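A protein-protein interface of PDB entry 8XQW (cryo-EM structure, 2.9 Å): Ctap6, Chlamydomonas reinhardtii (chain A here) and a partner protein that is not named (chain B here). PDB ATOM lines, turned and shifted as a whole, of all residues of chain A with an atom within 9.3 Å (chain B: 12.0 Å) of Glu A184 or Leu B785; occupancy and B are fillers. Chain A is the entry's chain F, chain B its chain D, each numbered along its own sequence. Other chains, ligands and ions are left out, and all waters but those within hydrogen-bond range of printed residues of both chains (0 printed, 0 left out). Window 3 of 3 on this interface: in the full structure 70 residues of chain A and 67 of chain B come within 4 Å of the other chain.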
ATOM      1  N   TYR A 113     -23.071  35.435 -18.171  1.00  0.00           N
ATOM      2  CA  TYR A 113     -23.773  34.445 -18.978  1.00  0.00           C
ATOM      3  C   TYR A 113     -24.895  35.080 -19.784  1.00  0.00           C
ATOM      4  O   TYR A 113     -24.971  34.900 -21.006  1.00  0.00           O
ATOM      5  CB  TYR A 113     -24.309  33.341 -18.074  1.00  0.00           C
ATOM      6  CG  TYR A 113     -25.238  32.381 -18.760  1.00  0.00           C
ATOM      7  CD1 TYR A 113     -24.754  31.443 -19.651  1.00  0.00           C
ATOM      8  CD2 TYR A 113     -26.597  32.407 -18.508  1.00  0.00           C
ATOM      9  CE1 TYR A 113     -25.596  30.565 -20.273  1.00  0.00           C
ATOM     10  CE2 TYR A 113     -27.445  31.532 -19.122  1.00  0.00           C
ATOM     11  CZ  TYR A 113     -26.941  30.613 -20.007  1.00  0.00           C
ATOM     12  OH  TYR A 113     -27.786  29.732 -20.631  1.00  0.00           O
ATOM     13  N   GLY A 114     -25.787  35.816 -19.122  1.00  0.00           N
ATOM     14  CA  GLY A 114     -26.844  36.497 -19.848  1.00  0.00           C
ATOM     15  C   GLY A 114     -26.298  37.517 -20.824  1.00  0.00           C
ATOM     16  O   GLY A 114     -26.864  37.730 -21.900  1.00  0.00           O
ATOM     17  N   VAL A 116     -23.422  37.236 -22.516  1.00  0.00           N
ATOM     18  CA  VAL A 116     -22.973  36.493 -23.687  1.00  0.00           C
ATOM     19  C   VAL A 116     -24.161  36.035 -24.516  1.00  0.00           C
ATOM     20  O   VAL A 116     -24.131  36.083 -25.750  1.00  0.00           O
ATOM     21  CB  VAL A 116     -22.097  35.306 -23.257  1.00  0.00           C
ATOM     22  CG1 VAL A 116     -22.047  34.273 -24.346  1.00  0.00           C
ATOM     23  CG2 VAL A 116     -20.709  35.780 -22.932  1.00  0.00           C
ATOM     24  N   LEU A 117     -25.228  35.586 -23.857  1.00  0.00           N
ATOM     25  CA  LEU A 117     -26.408  35.157 -24.595  1.00  0.00           C
ATOM     26  C   LEU A 117     -26.990  36.297 -25.418  1.00  0.00           C
ATOM     27  O   LEU A 117     -27.318  36.116 -26.596  1.00  0.00           O
ATOM     28  CB  LEU A 117     -27.452  34.609 -23.632  1.00  0.00           C
ATOM     29  CG  LEU A 117     -28.668  33.989 -24.297  1.00  0.00           C
ATOM     30  CD1 LEU A 117     -28.235  33.047 -25.387  1.00  0.00           C
ATOM     31  CD2 LEU A 117     -29.474  33.266 -23.261  1.00  0.00           C
ATOM     32  N   TRP A 130     -12.925  28.237 -27.107  1.00  0.00           N
ATOM     33  CA  TRP A 130     -12.693  27.513 -25.869  1.00  0.00           C
ATOM     34  C   TRP A 130     -11.256  27.029 -25.798  1.00  0.00           C
ATOM     35  O   TRP A 130     -10.619  26.783 -26.820  1.00  0.00           O
ATOM     36  CB  TRP A 130     -13.625  26.311 -25.736  1.00  0.00           C
ATOM     37  CG  TRP A 130     -15.003  26.543 -26.226  1.00  0.00           C
ATOM     38  CD1 TRP A 130     -15.429  26.512 -27.516  1.00  0.00           C
ATOM     39  CD2 TRP A 130     -16.150  26.823 -25.433  1.00  0.00           C
ATOM     40  NE1 TRP A 130     -16.772  26.765 -27.580  1.00  0.00           N
ATOM     41  CE2 TRP A 130     -17.237  26.962 -26.310  1.00  0.00           C
ATOM     42  CE3 TRP A 130     -16.362  26.977 -24.069  1.00  0.00           C
ATOM     43  CZ2 TRP A 130     -18.509  27.244 -25.867  1.00  0.00           C
ATOM     44  CZ3 TRP A 130     -17.621  27.255 -23.636  1.00  0.00           C
ATOM     45  CH2 TRP A 130     -18.683  27.387 -24.530  1.00  0.00           C
ATOM     46  N   PRO A 162     -12.749  21.344 -19.515  1.00  0.00           N
ATOM     47  CA  PRO A 162     -13.802  21.022 -18.548  1.00  0.00           C
ATOM     48  C   PRO A 162     -14.191  22.189 -17.673  1.00  0.00           C
ATOM     49  O   PRO A 162     -15.357  22.278 -17.282  1.00  0.00           O
ATOM     50  CB  PRO A 162     -13.184  19.893 -17.719  1.00  0.00           C
ATOM     51  CG  PRO A 162     -12.104  19.358 -18.557  1.00  0.00           C
ATOM     52  CD  PRO A 162     -11.560  20.509 -19.320  1.00  0.00           C
ATOM     53  N   ASP A 163     -13.267  23.089 -17.358  1.00  0.00           N
ATOM     54  CA  ASP A 163     -13.563  24.224 -16.500  1.00  0.00           C
ATOM     55  C   ASP A 163     -14.372  25.301 -17.196  1.00  0.00           C
ATOM     56  O   ASP A 163     -14.833  26.230 -16.533  1.00  0.00           O
ATOM     57  CB  ASP A 163     -12.271  24.826 -15.962  1.00  0.00           C
ATOM     58  CG  ASP A 163     -11.206  24.930 -17.015  1.00  0.00           C
ATOM     59  OD1 ASP A 163     -11.551  24.905 -18.209  1.00  0.00           O
ATOM     60  OD2 ASP A 163     -10.019  25.041 -16.655  1.00  0.00           O
ATOM     61  N   GLY A 164     -14.556  25.209 -18.503  1.00  0.00           N
ATOM     62  CA  GLY A 164     -15.391  26.168 -19.183  1.00  0.00           C
ATOM     63  C   GLY A 164     -14.763  27.510 -19.447  1.00  0.00           C
ATOM     64  O   GLY A 164     -15.489  28.459 -19.744  1.00  0.00           O
ATOM     65  N   VAL A 179     -16.883  32.139 -18.326  1.00  0.00           N
ATOM     66  CA  VAL A 179     -16.952  30.737 -17.943  1.00  0.00           C
ATOM     67  C   VAL A 179     -18.276  30.202 -18.457  1.00  0.00           C
ATOM     68  O   VAL A 179     -19.346  30.636 -18.017  1.00  0.00           O
ATOM     69  CB  VAL A 179     -16.818  30.539 -16.431  1.00  0.00           C
ATOM     70  CG1 VAL A 179     -17.448  29.236 -16.019  1.00  0.00           C
ATOM     71  CG2 VAL A 179     -15.366  30.544 -16.033  1.00  0.00           C
ATOM     72  N   ILE A 180     -18.207  29.282 -19.411  1.00  0.00           N
ATOM     73  CA  ILE A 180     -19.396  28.677 -19.995  1.00  0.00           C
ATOM     74  C   ILE A 180     -19.143  27.184 -20.117  1.00  0.00           C
ATOM     75  O   ILE A 180     -18.147  26.781 -20.727  1.00  0.00           O
ATOM     76  CB  ILE A 180     -19.729  29.283 -21.361  1.00  0.00           C
ATOM     77  CG1 ILE A 180     -20.214  30.713 -21.211  1.00  0.00           C
ATOM     78  CG2 ILE A 180     -20.792  28.474 -22.040  1.00  0.00           C
ATOM     79  CD1 ILE A 180     -20.177  31.465 -22.494  1.00  0.00           C
ATOM     80  N   PRO A 181     -19.988  26.336 -19.555  1.00  0.00           N
ATOM     81  CA  PRO A 181     -19.789  24.909 -19.693  1.00  0.00           C
ATOM     82  C   PRO A 181     -20.076  24.473 -21.114  1.00  0.00           C
ATOM     83  O   PRO A 181     -21.093  24.872 -21.695  1.00  0.00           O
ATOM     84  CB  PRO A 181     -20.809  24.313 -18.716  1.00  0.00           C
ATOM     85  CG  PRO A 181     -21.240  25.433 -17.870  1.00  0.00           C
ATOM     86  CD  PRO A 181     -21.141  26.642 -18.706  1.00  0.00           C
ATOM     87  N   PRO A 182     -19.202  23.669 -21.712  1.00  0.00           N
ATOM     88  CA  PRO A 182     -19.494  23.154 -23.053  1.00  0.00           C
ATOM     89  C   PRO A 182     -20.715  22.253 -23.004  1.00  0.00           C
ATOM     90  O   PRO A 182     -20.746  21.269 -22.265  1.00  0.00           O
ATOM     91  CB  PRO A 182     -18.228  22.373 -23.422  1.00  0.00           C
ATOM     92  CG  PRO A 182     -17.208  22.762 -22.415  1.00  0.00           C
ATOM     93  CD  PRO A 182     -17.938  23.144 -21.184  1.00  0.00           C
ATOM     94  N   GLY A 183     -21.731  22.608 -23.779  1.00  0.00           N
ATOM     95  CA  GLY A 183     -22.969  21.865 -23.783  1.00  0.00           C
ATOM     96  C   GLY A 183     -24.094  22.484 -22.987  1.00  0.00           C
ATOM     97  O   GLY A 183     -25.067  21.788 -22.684  1.00  0.00           O
ATOM     98  N   GLU A 184     -23.989  23.751 -22.625  1.00  0.00           N
ATOM     99  CA  GLU A 184     -25.113  24.431 -22.010  1.00  0.00           C
ATOM    100  C   GLU A 184     -26.239  24.547 -23.028  1.00  0.00           C
ATOM    101  O   GLU A 184     -25.977  24.857 -24.195  1.00  0.00           O
ATOM    102  CB  GLU A 184     -24.689  25.811 -21.524  1.00  0.00           C
ATOM    103  CG  GLU A 184     -25.234  26.180 -20.171  1.00  0.00           C
ATOM    104  CD  GLU A 184     -26.554  26.906 -20.266  1.00  0.00           C
ATOM    105  OE1 GLU A 184     -27.477  26.581 -19.496  1.00  0.00           O
ATOM    106  OE2 GLU A 184     -26.671  27.809 -21.118  1.00  0.00           O
ATOM    107  N   PRO A 185     -27.483  24.302 -22.643  1.00  0.00           N
ATOM    108  CA  PRO A 185     -28.570  24.239 -23.630  1.00  0.00           C
ATOM    109  C   PRO A 185     -28.814  25.535 -24.395  1.00  0.00           C
ATOM    110  O   PRO A 185     -28.821  25.526 -25.629  1.00  0.00           O
ATOM    111  CB  PRO A 185     -29.786  23.860 -22.781  1.00  0.00           C
ATOM    112  CG  PRO A 185     -29.395  24.150 -21.387  1.00  0.00           C
ATOM    113  CD  PRO A 185     -27.941  23.923 -21.303  1.00  0.00           C
ATOM    114  N   ARG A 186     -29.021  26.646 -23.685  1.00  0.00           N
ATOM    115  CA  ARG A 186     -29.335  27.906 -24.353  1.00  0.00           C
ATOM    116  C   ARG A 186     -28.207  28.341 -25.274  1.00  0.00           C
ATOM    117  O   ARG A 186     -28.441  28.705 -26.431  1.00  0.00           O
ATOM    118  CB  ARG A 186     -29.614  28.992 -23.324  1.00  0.00           C
ATOM    119  CG  ARG A 186     -31.025  29.018 -22.825  1.00  0.00           C
ATOM    120  CD  ARG A 186     -31.968  29.595 -23.837  1.00  0.00           C
ATOM    121  NE  ARG A 186     -33.340  29.443 -23.384  1.00  0.00           N
ATOM    122  CZ  ARG A 186     -34.393  29.478 -24.184  1.00  0.00           C
ATOM    123  NH1 ARG A 186     -35.611  29.321 -23.696  1.00  0.00           N
ATOM    124  NH2 ARG A 186     -34.225  29.671 -25.480  1.00  0.00           N
ATOM    125  N   ILE A 187     -26.975  28.331 -24.772  1.00  0.00           N
ATOM    126  CA  ILE A 187     -25.850  28.787 -25.579  1.00  0.00           C
ATOM    127  C   ILE A 187     -25.652  27.876 -26.778  1.00  0.00           C
ATOM    128  O   ILE A 187     -25.329  28.338 -27.877  1.00  0.00           O
ATOM    129  CB  ILE A 187     -24.581  28.869 -24.718  1.00  0.00           C
ATOM    130  CG1 ILE A 187     -24.759  29.911 -23.625  1.00  0.00           C
ATOM    131  CG2 ILE A 187     -23.393  29.233 -25.565  1.00  0.00           C
ATOM    132  CD1 ILE A 187     -24.878  31.297 -24.149  1.00  0.00           C
ATOM    133  N   SER A 188     -25.854  26.574 -26.599  1.00  0.00           N
ATOM    134  CA  SER A 188     -25.696  25.655 -27.716  1.00  0.00           C
ATOM    135  C   SER A 188     -26.729  25.929 -28.797  1.00  0.00           C
ATOM    136  O   SER A 188     -26.398  26.003 -29.986  1.00  0.00           O
ATOM    137  CB  SER A 188     -25.801  24.218 -27.228  1.00  0.00           C
ATOM    138  OG  SER A 188     -24.992  24.032 -26.087  1.00  0.00           O
ATOM    139  N   GLN A 189     -27.993  26.082 -28.404  1.00  0.00           N
ATOM    140  CA  GLN A 189     -29.020  26.395 -29.387  1.00  0.00           C
ATOM    141  C   GLN A 189     -28.723  27.709 -30.089  1.00  0.00           C
ATOM    142  O   GLN A 189     -28.908  27.823 -31.304  1.00  0.00           O
ATOM    143  CB  GLN A 189     -30.388  26.450 -28.722  1.00  0.00           C
ATOM    144  CG  GLN A 189     -30.941  25.107 -28.340  1.00  0.00           C
ATOM    145  CD  GLN A 189     -32.360  25.204 -27.850  1.00  0.00           C
ATOM    146  OE1 GLN A 189     -32.917  26.292 -27.745  1.00  0.00           O
ATOM    147  NE2 GLN A 189     -32.963  24.064 -27.555  1.00  0.00           N
ATOM    148  N   ALA A 190     -28.256  28.712 -29.348  1.00  0.00           N
ATOM    149  CA  ALA A 190     -27.965  29.993 -29.972  1.00  0.00           C
ATOM    150  C   ALA A 190     -26.841  29.868 -30.987  1.00  0.00           C
ATOM    151  O   ALA A 190     -26.933  30.410 -32.091  1.00  0.00           O
ATOM    152  CB  ALA A 190     -27.615  31.029 -28.910  1.00  0.00           C
ATOM    153  N   LEU A 191     -25.778  29.149 -30.637  1.00  0.00           N
ATOM    154  CA  LEU A 191     -24.662  29.004 -31.561  1.00  0.00           C
ATOM    155  C   LEU A 191     -25.060  28.195 -32.786  1.00  0.00           C
ATOM    156  O   LEU A 191     -24.551  28.432 -33.884  1.00  0.00           O
ATOM    157  CB  LEU A 191     -23.476  28.355 -30.859  1.00  0.00           C
ATOM    158  CG  LEU A 191     -22.834  29.238 -29.800  1.00  0.00           C
ATOM    159  CD1 LEU A 191     -21.976  28.415 -28.885  1.00  0.00           C
ATOM    160  CD2 LEU A 191     -22.018  30.313 -30.456  1.00  0.00           C
ATOM    161  N   GLN A 192     -25.970  27.235 -32.622  1.00  0.00           N
ATOM    162  CA  GLN A 192     -26.405  26.456 -33.775  1.00  0.00           C
ATOM    163  C   GLN A 192     -27.311  27.275 -34.681  1.00  0.00           C
ATOM    164  O   GLN A 192     -27.278  27.126 -35.906  1.00  0.00           O
ATOM    165  CB  GLN A 192     -27.110  25.181 -33.324  1.00  0.00           C
ATOM    166  CG  GLN A 192     -26.219  24.236 -32.544  1.00  0.00           C
ATOM    167  CD  GLN A 192     -26.413  22.787 -32.934  1.00  0.00           C
ATOM    168  OE1 GLN A 192     -26.875  22.486 -34.032  1.00  0.00           O
ATOM    169  NE2 GLN A 192     -26.073  21.881 -32.026  1.00  0.00           N
ATOM    170  N   ASN B 782     -31.688  17.473 -23.267  1.00  0.00           N
ATOM    171  CA  ASN B 782     -31.236  18.324 -22.178  1.00  0.00           C
ATOM    172  C   ASN B 782     -29.835  18.874 -22.439  1.00  0.00           C
ATOM    173  O   ASN B 782     -29.577  19.489 -23.473  1.00  0.00           O
ATOM    174  CB  ASN B 782     -31.263  17.552 -20.862  1.00  0.00           C
ATOM    175  CG  ASN B 782     -31.215  18.458 -19.653  1.00  0.00           C
ATOM    176  OD1 ASN B 782     -30.339  19.313 -19.537  1.00  0.00           O
ATOM    177  ND2 ASN B 782     -32.159  18.276 -18.742  1.00  0.00           N
ATOM    178  N   GLY B 783     -28.939  18.636 -21.492  1.00  0.00           N
ATOM    179  CA  GLY B 783     -27.580  19.135 -21.542  1.00  0.00           C
ATOM    180  C   GLY B 783     -27.081  19.406 -20.143  1.00  0.00           C
ATOM    181  O   GLY B 783     -27.763  20.013 -19.319  1.00  0.00           O
ATOM    182  N   HIS B 784     -25.865  18.935 -19.875  1.00  0.00           N
ATOM    183  CA  HIS B 784     -25.374  18.876 -18.505  1.00  0.00           C
ATOM    184  C   HIS B 784     -24.408  20.011 -18.207  1.00  0.00           C
ATOM    185  O   HIS B 784     -23.833  20.625 -19.109  1.00  0.00           O
ATOM    186  CB  HIS B 784     -24.711  17.537 -18.191  1.00  0.00           C
ATOM    187  CG  HIS B 784     -25.502  16.707 -17.232  1.00  0.00           C
ATOM    188  ND1 HIS B 784     -26.731  17.106 -16.752  1.00  0.00           N
ATOM    189  CD2 HIS B 784     -25.247  15.508 -16.662  1.00  0.00           C
ATOM    190  CE1 HIS B 784     -27.200  16.187 -15.931  1.00  0.00           C
ATOM    191  NE2 HIS B 784     -26.318  15.207 -15.856  1.00  0.00           N
ATOM    192  N   LEU B 785     -24.243  20.272 -16.908  1.00  0.00           N
ATOM    193  CA  LEU B 785     -23.638  21.511 -16.446  1.00  0.00           C
ATOM    194  C   LEU B 785     -22.496  21.298 -15.463  1.00  0.00           C
ATOM    195  O   LEU B 785     -22.176  22.220 -14.708  1.00  0.00           O
ATOM    196  CB  LEU B 785     -24.707  22.389 -15.804  1.00  0.00           C
ATOM    197  CG  LEU B 785     -25.954  22.551 -16.668  1.00  0.00           C
ATOM    198  CD1 LEU B 785     -27.056  23.256 -15.920  1.00  0.00           C
ATOM    199  CD2 LEU B 785     -25.597  23.304 -17.927  1.00  0.00           C
ATOM    200  N   SER B 786     -21.873  20.126 -15.443  1.00  0.00           N
ATOM    201  CA  SER B 786     -20.748  19.902 -14.551  1.00  0.00           C
ATOM    202  C   SER B 786     -19.552  20.732 -14.990  1.00  0.00           C
ATOM    203  O   SER B 786     -19.260  20.848 -16.180  1.00  0.00           O
ATOM    204  CB  SER B 786     -20.364  18.426 -14.526  1.00  0.00           C
ATOM    205  OG  SER B 786     -19.199  18.205 -15.301  1.00  0.00           O
ATOM    206  N   VAL B 787     -18.859  21.308 -14.020  1.00  0.00           N
ATOM    207  CA  VAL B 787     -17.690  22.129 -14.271  1.00  0.00           C
ATOM    208  C   VAL B 787     -16.635  21.779 -13.235  1.00  0.00           C
ATOM    209  O   VAL B 787     -16.924  21.676 -12.042  1.00  0.00           O
ATOM    210  CB  VAL B 787     -18.037  23.630 -14.220  1.00  0.00           C
ATOM    211  CG1 VAL B 787     -16.796  24.459 -14.093  1.00  0.00           C
ATOM    212  CG2 VAL B 787     -18.783  24.030 -15.453  1.00  0.00           C
ATOM    213  N   VAL B 788     -15.416  21.565 -13.700  1.00  0.00           N
ATOM    214  CA  VAL B 788     -14.277  21.347 -12.826  1.00  0.00           C
ATOM    215  C   VAL B 788     -13.605  22.691 -12.608  1.00  0.00           C
ATOM    216  O   VAL B 788     -13.670  23.573 -13.464  1.00  0.00           O
ATOM    217  CB  VAL B 788     -13.304  20.320 -13.431  1.00  0.00           C
ATOM    218  CG1 VAL B 788     -12.355  19.809 -12.390  1.00  0.00           C
ATOM    219  CG2 VAL B 788     -14.075  19.177 -14.027  1.00  0.00           C
ATOM    220  N   SER B 789     -12.978  22.864 -11.448  1.00  0.00           N
ATOM    221  CA  SER B 789     -12.379  24.160 -11.148  1.00  0.00           C
ATOM    222  C   SER B 789     -11.085  24.362 -11.919  1.00  0.00           C
ATOM    223  O   SER B 789     -10.857  25.432 -12.493  1.00  0.00           O
ATOM    224  CB  SER B 789     -12.133  24.291  -9.651  1.00  0.00           C
ATOM    225  OG  SER B 789     -11.907  25.639  -9.293  1.00  0.00           O
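Of chain B, only Leu B785 (3.7 Å) comes within 4 Å of Glu A184. Leu B785 touches just one residue of chain A: Glu A184. No residue of chain B comes within 4 Å of Ile A180. No residue of chain B comes within 4 Å of Pro A185. No residue of chain B comes within 4 Å of Ile A187. No residue of chain A comes within 4 Å of Ser B786. Printed residues of chain B within 4 Å of Pro A162: Val B787 and Val B788. Printed residues of chain A within 4 Å of Val B787: Pro A162, Asp A163 and Pro A181. Printed residues of chain B within 4 Å of Asp A163: Val B787 (3.6 Å), Val B788 (3.1 Å) and Ser B789 (3.8 Å). Printed residues of chain A within 4 Å of Gly B783: Gly A183. Tyr A113 touches none of the printed residues of chain B. The nearest residue of chain A that does not touch Leu B785 is Pro A185 (4.2 Å). The nearest printed residue of chain A that does not touch His B784 is Pro A182 (4.5 Å).
The side-chain carboxylate (OE1) of Glu A184 lies close to the side-chain hydroxyl (OH) of Tyr A113 (3.4 Å).
Hydrophobic or aromatic side chains of chain A within 4 Å of the printed part of chain B: Pro A162 and Pro A181. Printed residues of chain B that touch a printed residue of chain A: Gly B783, His B784, Leu B785, Val B787, Val B788 and Ser B789. Hydrophobic or aromatic side chains of chain B that line the printed part of chain A: Leu B785, Val B787 and Val B788. Among the printed residues, 9 pairs touch across the chains.
Pro A162 touches Val B787. Pro A162 touches Val B788. Asp A163 touches Val B787. Asp A163 touches Val B788. Asp A163 touches Ser B789. Val B787 touches Pro A181 (CG2 to CG, 3.7 Å). Gly B783 touches Gly A183 (CA to O, 3.8 Å). O of Gly A183 touches O of His B784, at 3.96 Å. CG of Glu A184 touches CD2 of Leu B785, 3.7 Å away.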
